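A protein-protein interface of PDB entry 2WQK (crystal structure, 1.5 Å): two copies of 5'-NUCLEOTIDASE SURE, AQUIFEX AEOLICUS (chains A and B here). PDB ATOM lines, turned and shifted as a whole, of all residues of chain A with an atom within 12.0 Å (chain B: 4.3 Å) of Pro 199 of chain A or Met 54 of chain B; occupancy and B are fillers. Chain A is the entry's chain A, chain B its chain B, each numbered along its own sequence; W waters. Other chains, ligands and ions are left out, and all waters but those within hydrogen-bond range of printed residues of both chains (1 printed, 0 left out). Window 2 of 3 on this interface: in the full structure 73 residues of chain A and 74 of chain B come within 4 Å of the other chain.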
ATOM      1  N   GLU A 187      35.730  10.954  -2.467  1.00  0.00           N
ATOM      2  CA  GLU A 187      34.651  11.559  -1.704  1.00  0.00           C
ATOM      3  C   GLU A 187      35.216  12.429  -0.582  1.00  0.00           C
ATOM      4  O   GLU A 187      36.038  11.994   0.208  1.00  0.00           O
ATOM      5  CB  GLU A 187      33.765  10.446  -1.150  1.00  0.00           C
ATOM      6  CG  GLU A 187      32.589  10.887  -0.350  1.00  0.00           C
ATOM      7  CD  GLU A 187      31.604   9.739  -0.142  1.00  0.00           C
ATOM      8  OE1 GLU A 187      31.684   9.077   0.896  1.00  0.00           O
ATOM      9  OE2 GLU A 187      30.776   9.468  -1.047  1.00  0.00           O
ATOM     10  N   ARG A 188      34.735  13.660  -0.507  1.00  0.00           N
ATOM     11  CA  ARG A 188      35.109  14.572   0.570  1.00  0.00           C
ATOM     12  C   ARG A 188      33.845  15.235   1.107  1.00  0.00           C
ATOM     13  O   ARG A 188      33.020  15.675   0.308  1.00  0.00           O
ATOM     14  CB  ARG A 188      36.044  15.649   0.021  1.00  0.00           C
ATOM     15  CG  ARG A 188      36.869  16.369   1.059  1.00  0.00           C
ATOM     16  CD  ARG A 188      37.458  17.669   0.458  1.00  0.00           C
ATOM     17  NE  ARG A 188      38.181  18.581   1.367  1.00  0.00           N
ATOM     18  CZ  ARG A 188      37.771  19.043   2.555  1.00  0.00           C
ATOM     19  NH1 ARG A 188      36.623  18.677   3.118  1.00  0.00           N
ATOM     20  NH2 ARG A 188      38.560  19.891   3.217  1.00  0.00           N
ATOM     21  N   VAL A 189      33.707  15.316   2.427  1.00  0.00           N
ATOM     22  CA  VAL A 189      32.543  15.971   3.046  1.00  0.00           C
ATOM     23  C   VAL A 189      32.960  17.345   3.550  1.00  0.00           C
ATOM     24  O   VAL A 189      34.007  17.493   4.224  1.00  0.00           O
ATOM     25  CB  VAL A 189      31.939  15.132   4.200  1.00  0.00           C
ATOM     26  CG1 VAL A 189      30.768  15.850   4.819  1.00  0.00           C
ATOM     27  CG2 VAL A 189      31.557  13.731   3.686  1.00  0.00           C
ATOM     28  N   PHE A 190      32.189  18.351   3.158  1.00  0.00           N
ATOM     29  CA  PHE A 190      32.424  19.757   3.569  1.00  0.00           C
ATOM     30  C   PHE A 190      31.390  20.089   4.645  1.00  0.00           C
ATOM     31  O   PHE A 190      30.233  19.718   4.512  1.00  0.00           O
ATOM     32  CB  PHE A 190      32.280  20.691   2.380  1.00  0.00           C
ATOM     33  CG  PHE A 190      33.395  20.552   1.354  1.00  0.00           C
ATOM     34  CD1 PHE A 190      34.447  21.452   1.335  1.00  0.00           C
ATOM     35  CD2 PHE A 190      33.399  19.512   0.431  1.00  0.00           C
ATOM     36  CE1 PHE A 190      35.481  21.321   0.408  1.00  0.00           C
ATOM     37  CE2 PHE A 190      34.431  19.368  -0.501  1.00  0.00           C
ATOM     38  CZ  PHE A 190      35.473  20.284  -0.517  1.00  0.00           C
ATOM     39  N   LYS A 191      31.812  20.771   5.708  1.00  0.00           N
ATOM     40  CA  LYS A 191      30.953  21.157   6.808  1.00  0.00           C
ATOM     41  C   LYS A 191      30.673  22.661   6.724  1.00  0.00           C
ATOM     42  O   LYS A 191      31.592  23.479   6.470  1.00  0.00           O
ATOM     43  CB  LYS A 191      31.620  20.875   8.170  1.00  0.00           C
ATOM     44  CG  LYS A 191      30.712  21.094   9.356  1.00  0.00           C
ATOM     45  CD  LYS A 191      31.366  20.660  10.659  1.00  0.00           C
ATOM     46  CE  LYS A 191      30.465  20.900  11.848  1.00  0.00           C
ATOM     47  NZ  LYS A 191      31.200  20.574  13.139  1.00  0.00           N
ATOM     48  N   TYR A 192      29.424  22.995   7.009  1.00  0.00           N
ATOM     49  CA  TYR A 192      28.933  24.369   7.065  1.00  0.00           C
ATOM     50  C   TYR A 192      28.154  24.567   8.346  1.00  0.00           C
ATOM     51  O   TYR A 192      27.743  23.576   8.989  1.00  0.00           O
ATOM     52  CB  TYR A 192      28.016  24.632   5.886  1.00  0.00           C
ATOM     53  CG  TYR A 192      28.662  24.520   4.526  1.00  0.00           C
ATOM     54  CD1 TYR A 192      29.167  25.626   3.874  1.00  0.00           C
ATOM     55  CD2 TYR A 192      28.716  23.305   3.868  1.00  0.00           C
ATOM     56  CE1 TYR A 192      29.718  25.512   2.598  1.00  0.00           C
ATOM     57  CE2 TYR A 192      29.274  23.187   2.612  1.00  0.00           C
ATOM     58  CZ  TYR A 192      29.762  24.300   1.975  1.00  0.00           C
ATOM     59  OH  TYR A 192      30.291  24.178   0.721  1.00  0.00           O
ATOM     60  N   ILE A 193      27.911  25.837   8.706  1.00  0.00           N
ATOM     61  CA  ILE A 193      26.985  26.163   9.800  1.00  0.00           C
ATOM     62  C   ILE A 193      25.791  26.979   9.301  1.00  0.00           C
ATOM     63  O   ILE A 193      25.976  27.959   8.579  1.00  0.00           O
ATOM     64  CB  ILE A 193      27.718  26.894  10.946  1.00  0.00           C
ATOM     65  CG1 ILE A 193      28.906  26.056  11.426  1.00  0.00           C
ATOM     66  CG2 ILE A 193      26.751  27.216  12.071  1.00  0.00           C
ATOM     67  CD1 ILE A 193      28.498  24.807  12.192  1.00  0.00           C
ATOM     68  N   ASP A 194      24.572  26.531   9.610  1.00  0.00           N
ATOM     69  CA  ASP A 194      23.373  27.199   9.111  1.00  0.00           C
ATOM     70  C   ASP A 194      23.126  28.524   9.875  1.00  0.00           C
ATOM     71  O   ASP A 194      23.821  28.831  10.843  1.00  0.00           O
ATOM     72  CB  ASP A 194      22.150  26.241   9.064  1.00  0.00           C
ATOM     73  CG  ASP A 194      21.518  25.969  10.438  1.00  0.00           C
ATOM     74  OD1 ASP A 194      21.701  26.769  11.393  1.00  0.00           O
ATOM     75  OD2 ASP A 194      20.788  24.948  10.558  1.00  0.00           O
ATOM     76  N   PRO A 195      22.158  29.336   9.417  1.00  0.00           N
ATOM     77  CA  PRO A 195      21.874  30.628  10.056  1.00  0.00           C
ATOM     78  C   PRO A 195      21.478  30.603  11.520  1.00  0.00           C
ATOM     79  O   PRO A 195      21.518  31.674  12.176  1.00  0.00           O
ATOM     80  CB  PRO A 195      20.706  31.157   9.215  1.00  0.00           C
ATOM     81  CG  PRO A 195      20.883  30.496   7.899  1.00  0.00           C
ATOM     82  CD  PRO A 195      21.330  29.144   8.205  1.00  0.00           C
ATOM     83  N   TYR A 196      21.101  29.416  12.008  1.00  0.00           N
ATOM     84  CA  TYR A 196      20.660  29.188  13.398  1.00  0.00           C
ATOM     85  C   TYR A 196      21.758  28.501  14.231  1.00  0.00           C
ATOM     86  O   TYR A 196      21.501  28.095  15.364  1.00  0.00           O
ATOM     87  CB  TYR A 196      19.368  28.363  13.384  1.00  0.00           C
ATOM     88  CG  TYR A 196      18.370  28.865  12.360  1.00  0.00           C
ATOM     89  CD1 TYR A 196      17.744  30.100  12.520  1.00  0.00           C
ATOM     90  CD2 TYR A 196      18.078  28.130  11.209  1.00  0.00           C
ATOM     91  CE1 TYR A 196      16.844  30.592  11.543  1.00  0.00           C
ATOM     92  CE2 TYR A 196      17.164  28.611  10.233  1.00  0.00           C
ATOM     93  CZ  TYR A 196      16.558  29.842  10.412  1.00  0.00           C
ATOM     94  OH  TYR A 196      15.658  30.309   9.438  1.00  0.00           O
ATOM     95  N   GLY A 197      22.964  28.357  13.669  1.00  0.00           N
ATOM     96  CA  GLY A 197      24.114  27.763  14.376  1.00  0.00           C
ATOM     97  C   GLY A 197      24.269  26.252  14.350  1.00  0.00           C
ATOM     98  O   GLY A 197      25.125  25.698  15.077  1.00  0.00           O
ATOM     99  N   LYS A 198      23.477  25.579  13.505  1.00  0.00           N
ATOM    100  CA  LYS A 198      23.467  24.122  13.453  1.00  0.00           C
ATOM    101  C   LYS A 198      24.199  23.616  12.193  1.00  0.00           C
ATOM    102  O   LYS A 198      24.134  24.257  11.131  1.00  0.00           O
ATOM    103  CB  LYS A 198      22.033  23.588  13.465  1.00  0.00           C
ATOM    104  CG  LYS A 198      21.137  24.053  14.593  1.00  0.00           C
ATOM    105  CD  LYS A 198      21.474  23.323  15.868  1.00  0.00           C
ATOM    106  CE  LYS A 198      20.838  24.009  17.092  1.00  0.00           C
ATOM    107  NZ  LYS A 198      21.738  23.903  18.308  1.00  0.00           N
ATOM    108  N   PRO A 199      24.882  22.467  12.308  1.00  0.00           N
ATOM    109  CA  PRO A 199      25.722  21.983  11.219  1.00  0.00           C
ATOM    110  C   PRO A 199      24.978  21.388  10.049  1.00  0.00           C
ATOM    111  O   PRO A 199      23.915  20.764  10.199  1.00  0.00           O
ATOM    112  CB  PRO A 199      26.612  20.924  11.883  1.00  0.00           C
ATOM    113  CG  PRO A 199      25.765  20.386  12.980  1.00  0.00           C
ATOM    114  CD  PRO A 199      24.914  21.539  13.468  1.00  0.00           C
ATOM    115  N   PHE A 200      25.579  21.546   8.879  1.00  0.00           N
ATOM    116  CA  PHE A 200      25.116  20.805   7.699  1.00  0.00           C
ATOM    117  C   PHE A 200      26.313  20.481   6.817  1.00  0.00           C
ATOM    118  O   PHE A 200      27.410  21.028   7.001  1.00  0.00           O
ATOM    119  CB  PHE A 200      23.983  21.509   6.947  1.00  0.00           C
ATOM    120  CG  PHE A 200      24.373  22.806   6.266  1.00  0.00           C
ATOM    121  CD1 PHE A 200      24.557  22.844   4.891  1.00  0.00           C
ATOM    122  CD2 PHE A 200      24.467  24.005   6.960  1.00  0.00           C
ATOM    123  CE1 PHE A 200      24.879  24.032   4.234  1.00  0.00           C
ATOM    124  CE2 PHE A 200      24.780  25.204   6.290  1.00  0.00           C
ATOM    125  CZ  PHE A 200      24.955  25.212   4.937  1.00  0.00           C
ATOM    126  N   TYR A 201      26.121  19.539   5.904  1.00  0.00           N
ATOM    127  CA  TYR A 201      27.243  18.875   5.253  1.00  0.00           C
ATOM    128  C   TYR A 201      26.980  18.788   3.766  1.00  0.00           C
ATOM    129  O   TYR A 201      25.834  18.723   3.347  1.00  0.00           O
ATOM    130  CB  TYR A 201      27.450  17.456   5.832  1.00  0.00           C
ATOM    131  CG  TYR A 201      27.733  17.519   7.311  1.00  0.00           C
ATOM    132  CD1 TYR A 201      29.044  17.683   7.778  1.00  0.00           C
ATOM    133  CD2 TYR A 201      26.690  17.509   8.238  1.00  0.00           C
ATOM    134  CE1 TYR A 201      29.308  17.814   9.126  1.00  0.00           C
ATOM    135  CE2 TYR A 201      26.950  17.620   9.619  1.00  0.00           C
ATOM    136  CZ  TYR A 201      28.262  17.790  10.035  1.00  0.00           C
ATOM    137  OH  TYR A 201      28.509  17.880  11.410  1.00  0.00           O
ATOM    138  N   TRP A 202      28.029  18.764   2.976  1.00  0.00           N
ATOM    139  CA  TRP A 202      27.877  18.573   1.541  1.00  0.00           C
ATOM    140  C   TRP A 202      28.890  17.495   1.143  1.00  0.00           C
ATOM    141  O   TRP A 202      30.081  17.664   1.342  1.00  0.00           O
ATOM    142  CB  TRP A 202      28.151  19.888   0.784  1.00  0.00           C
ATOM    143  CG  TRP A 202      27.542  19.923  -0.597  1.00  0.00           C
ATOM    144  CD1 TRP A 202      27.593  18.948  -1.542  1.00  0.00           C
ATOM    145  CD2 TRP A 202      26.785  20.989  -1.151  1.00  0.00           C
ATOM    146  NE1 TRP A 202      26.898  19.330  -2.663  1.00  0.00           N
ATOM    147  CE2 TRP A 202      26.401  20.595  -2.463  1.00  0.00           C
ATOM    148  CE3 TRP A 202      26.399  22.236  -0.687  1.00  0.00           C
ATOM    149  CZ2 TRP A 202      25.612  21.417  -3.305  1.00  0.00           C
ATOM    150  CZ3 TRP A 202      25.648  23.062  -1.542  1.00  0.00           C
ATOM    151  CH2 TRP A 202      25.253  22.638  -2.819  1.00  0.00           C
ATOM    152  N   ILE A 203      28.382  16.386   0.618  1.00  0.00           N
ATOM    153  CA  ILE A 203      29.208  15.305   0.115  1.00  0.00           C
ATOM    154  C   ILE A 203      29.650  15.657  -1.302  1.00  0.00           C
ATOM    155  O   ILE A 203      28.809  15.805  -2.221  1.00  0.00           O
ATOM    156  CB  ILE A 203      28.467  13.958   0.101  1.00  0.00           C
ATOM    157  CG1 ILE A 203      27.844  13.658   1.477  1.00  0.00           C
ATOM    158  CG2 ILE A 203      29.416  12.860  -0.334  1.00  0.00           C
ATOM    159  CD1 ILE A 203      26.969  12.370   1.507  1.00  0.00           C
ATOM    160  N   VAL B  33      22.757   6.420  12.597  1.00  0.00           N
ATOM    161  CA  VAL B  33      22.558   7.582  11.734  1.00  0.00           C
ATOM    162  C   VAL B  33      21.447   7.171  10.769  1.00  0.00           C
ATOM    163  O   VAL B  33      21.609   6.205  10.032  1.00  0.00           O
ATOM    164  CB  VAL B  33      23.835   7.965  10.926  1.00  0.00           C
ATOM    165  CG1 VAL B  33      23.586   9.222  10.084  1.00  0.00           C
ATOM    166  CG2 VAL B  33      25.064   8.148  11.869  1.00  0.00           C
ATOM    167  N   LEU B  52      23.140  18.422   3.229  1.00  0.00           N
ATOM    168  CA  LEU B  52      22.332  17.617   4.123  1.00  0.00           C
ATOM    169  C   LEU B  52      22.503  18.107   5.559  1.00  0.00           C
ATOM    170  O   LEU B  52      23.617  18.211   6.030  1.00  0.00           O
ATOM    171  CB  LEU B  52      22.818  16.161   4.037  1.00  0.00           C
ATOM    172  CG  LEU B  52      22.583  15.459   2.691  1.00  0.00           C
ATOM    173  CD1 LEU B  52      23.412  14.186   2.610  1.00  0.00           C
ATOM    174  CD2 LEU B  52      21.128  15.197   2.500  1.00  0.00           C
ATOM    175  N   LYS B  53      21.387  18.377   6.219  1.00  0.00           N
ATOM    176  CA  LYS B  53      21.406  18.701   7.642  1.00  0.00           C
ATOM    177  C   LYS B  53      21.539  17.395   8.403  1.00  0.00           C
ATOM    178  O   LYS B  53      20.856  16.427   8.097  1.00  0.00           O
ATOM    179  CB  LYS B  53      20.128  19.397   8.063  1.00  0.00           C
ATOM    180  CG  LYS B  53      19.903  20.737   7.366  1.00  0.00           C
ATOM    181  CD  LYS B  53      18.768  21.522   8.023  1.00  0.00           C
ATOM    182  CE  LYS B  53      17.417  20.889   7.880  1.00  0.00           C
ATOM    183  NZ  LYS B  53      16.408  21.801   8.530  1.00  0.00           N
ATOM    184  N   MET B  54      22.380  17.403   9.424  1.00  0.00           N
ATOM    185  CA  MET B  54      22.453  16.229  10.310  1.00  0.00           C
ATOM    186  C   MET B  54      22.403  16.747  11.733  1.00  0.00           C
ATOM    187  O   MET B  54      23.170  17.674  12.087  1.00  0.00           O
ATOM    188  CB  MET B  54      23.704  15.350  10.002  1.00  0.00           C
ATOM    189  CG  MET B  54      23.812  14.061  10.895  1.00  0.00           C
ATOM    190  SD  MET B  54      25.161  12.977  10.399  1.00  0.00           S
ATOM    191  CE  MET B  54      26.629  13.990  10.274  1.00  0.00           C
ATOM    192  N   ARG B  55      21.470  16.166  12.493  1.00  0.00           N
ATOM    193  CA  ARG B  55      21.145  16.649  13.828  1.00  0.00           C
ATOM    194  C   ARG B  55      21.325  15.530  14.853  1.00  0.00           C
ATOM    195  O   ARG B  55      21.005  14.377  14.614  1.00  0.00           O
ATOM    196  CB  ARG B  55      19.706  17.160  13.848  1.00  0.00           C
ATOM    197  CG  ARG B  55      19.259  17.805  15.158  1.00  0.00           C
ATOM    198  CD  ARG B  55      17.805  18.316  15.118  1.00  0.00           C
ATOM    199  NE  ARG B  55      16.839  17.310  15.573  1.00  0.00           N
ATOM    200  CZ  ARG B  55      16.091  16.547  14.784  1.00  0.00           C
ATOM    201  NH1 ARG B  55      16.148  16.660  13.464  1.00  0.00           N
ATOM    202  NH2 ARG B  55      15.255  15.670  15.334  1.00  0.00           N
ATOM    203  N   TYR B  62      21.971  10.004  15.596  1.00  0.00           N
ATOM    204  CA  TYR B  62      21.887  11.160  14.690  1.00  0.00           C
ATOM    205  C   TYR B  62      20.853  10.911  13.618  1.00  0.00           C
ATOM    206  O   TYR B  62      20.581   9.765  13.251  1.00  0.00           O
ATOM    207  CB  TYR B  62      23.210  11.421  13.991  1.00  0.00           C
ATOM    208  CG  TYR B  62      24.313  11.824  14.931  1.00  0.00           C
ATOM    209  CD1 TYR B  62      24.651  13.166  15.100  1.00  0.00           C
ATOM    210  CD2 TYR B  62      25.019  10.855  15.627  1.00  0.00           C
ATOM    211  CE1 TYR B  62      25.677  13.530  16.011  1.00  0.00           C
ATOM    212  CE2 TYR B  62      26.028  11.209  16.522  1.00  0.00           C
ATOM    213  CZ  TYR B  62      26.359  12.536  16.699  1.00  0.00           C
ATOM    214  OH  TYR B  62      27.368  12.854  17.612  1.00  0.00           O
ATOM    215  N   THR B  63      20.261  11.998  13.145  1.00  0.00           N
ATOM    216  CA  THR B  63      19.389  11.892  11.975  1.00  0.00           C
ATOM    217  C   THR B  63      19.900  12.820  10.870  1.00  0.00           C
ATOM    218  O   THR B  63      20.398  13.910  11.148  1.00  0.00           O
ATOM    219  CB  THR B  63      17.900  12.205  12.287  1.00  0.00           C
ATOM    220  OG1 THR B  63      17.097  11.977  11.103  1.00  0.00           O
ATOM    221  CG2 THR B  63      17.691  13.647  12.808  1.00  0.00           C
ATOM    222  N   VAL B  64      19.739  12.343   9.627  1.00  0.00           N
ATOM    223  CA  VAL B  64      20.055  13.113   8.440  1.00  0.00           C
ATOM    224  C   VAL B  64      18.704  13.515   7.820  1.00  0.00           C
ATOM    225  O   VAL B  64      17.868  12.682   7.485  1.00  0.00           O
ATOM    226  CB  VAL B  64      20.947  12.328   7.403  1.00  0.00           C
ATOM    227  CG1 VAL B  64      21.287  13.241   6.190  1.00  0.00           C
ATOM    228  CG2 VAL B  64      22.253  11.830   8.045  1.00  0.00           C
ATOM    229  N   LEU B  75      27.861   9.685   5.678  1.00  0.00           N
ATOM    230  CA  LEU B  75      28.078  10.712   6.703  1.00  0.00           C
ATOM    231  C   LEU B  75      28.463  10.056   8.041  1.00  0.00           C
ATOM    232  O   LEU B  75      29.279  10.610   8.825  1.00  0.00           O
ATOM    233  CB  LEU B  75      26.860  11.601   6.901  1.00  0.00           C
ATOM    234  CG  LEU B  75      26.551  12.563   5.731  1.00  0.00           C
ATOM    235  CD1 LEU B  75      25.250  13.316   5.961  1.00  0.00           C
ATOM    236  CD2 LEU B  75      27.683  13.570   5.486  1.00  0.00           C
ATOM    237  N   VAL B  79      31.966  11.528   8.909  1.00  0.00           N
ATOM    238  CA  VAL B  79      31.801  12.628   9.882  1.00  0.00           C
ATOM    239  C   VAL B  79      31.733  12.046  11.302  1.00  0.00           C
ATOM    240  O   VAL B  79      32.622  12.308  12.136  1.00  0.00           O
ATOM    241  CB  VAL B  79      30.551  13.494   9.628  1.00  0.00           C
ATOM    242  CG1 VAL B  79      30.422  14.580  10.691  1.00  0.00           C
ATOM    243  CG2 VAL B  79      30.551  14.115   8.184  1.00  0.00           C
ATOM    244  N   ILE B  80      30.744  11.198  11.590  1.00  0.00           N
ATOM    245  CA  ILE B  80      30.500  10.795  12.973  1.00  0.00           C
ATOM    246  C   ILE B  80      31.663   9.923  13.499  1.00  0.00           C
ATOM    247  O   ILE B  80      32.171  10.145  14.605  1.00  0.00           O
ATOM    248  CB  ILE B  80      29.152  10.063  13.111  1.00  0.00           C
ATOM    249  CG1 ILE B  80      27.967  10.973  12.680  1.00  0.00           C
ATOM    250  CG2 ILE B  80      28.969   9.622  14.562  1.00  0.00           C
ATOM    251  CD1 ILE B  80      27.952  12.303  13.370  1.00  0.00           C
HETATM  252  O   HOH W   1      26.078  16.883  13.014  1.00  0.00           O
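The backbone carbonyl oxygen of Tyr 201 of chain A is in hydrogen-bond range of the backbone NH of Leu 52 of chain B, 2.7 Å away.
N of Tyr 192 of chain A sits at hydrogen-bond distance from O of Phe 200 of chain A (2.8 Å). N of Ile 80 of chain B lies within hydrogen-bond range of O of Leu 75 of chain B (3.2 Å).
No position is printed for both chains.
Water W1 lies within hydrogen-bond range of OH of Tyr 201 of chain A (3.1 Å) and O of Met 54 of chain B (3.2 Å).
Printed residues of chain B within 4 Å of Val 189 of chain A: Leu 75 (3.9 Å) and Val 79 (3.8 Å). Lys 191 of chain A touches none of the printed residues of chain B. Ile 193 of chain A touches none of the printed residues of chain B. Printed residues of chain B within 4 Å of Pro 199 of chain A: Met 54 (3.7 Å). Of the printed residues of chain B, Phe 200 of chain A touches Leu 52 (3.4 Å) and Lys 53 (3.9 Å). No residue of chain A comes within 4 Å of Val 33 of chain B. Of chain A, only Phe 200 (3.9 Å) comes within 4 Å of Lys 53 of chain B. Of the printed residues of chain A, Met 54 of chain B touches Pro 199 (3.7 Å) and Tyr 201 (3.7 Å). No residue of chain A comes within 4 Å of Thr 63 of chain B. No residue of chain A comes within 4 Å of Val 64 of chain B. The nearest printed residue of chain B that does not touch Pro 199 of chain A is Lys 53 of chain B (4.1 Å). The nearest residue of chain A that does not touch Met 54 of chain B is Phe 200 of chain A (4.7 Å).
Val 189 of chain A touches Leu 75 of chain B (CG1 to CD2, 3.9 Å). CG1 of Val 189 of chain A touches CG2 of Val 79 of chain B, 3.8 Å away. Met 54 of chain B touches Pro 199 of chain A (O to O, 3.7 Å). Leu 52 of chain B touches Phe 200 of chain A. Phe 200 of chain A touches Lys 53 of chain B (CB to CA, 3.9 Å). Tyr 201 of chain A touches Met 54 of chain B. Tyr 201 of chain A touches Leu 75 of chain B. Tyr 201 of chain A touches Val 79 of chain B (CE1 to CG1, 3.8 Å).
Of the 11 printed residues of chain B, 5 touch a printed residue of chain A. Printed residues of chain B that touch a printed residue of chain A: Leu 52, Lys 53, Met 54, Leu 75 and Val 79. Hydrophobic or aromatic side chains of chain B within 4 Å of the printed part of chain A: Met 54, Leu 75 and Val 79. Among the printed residues, 9 pairs touch across the chains.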
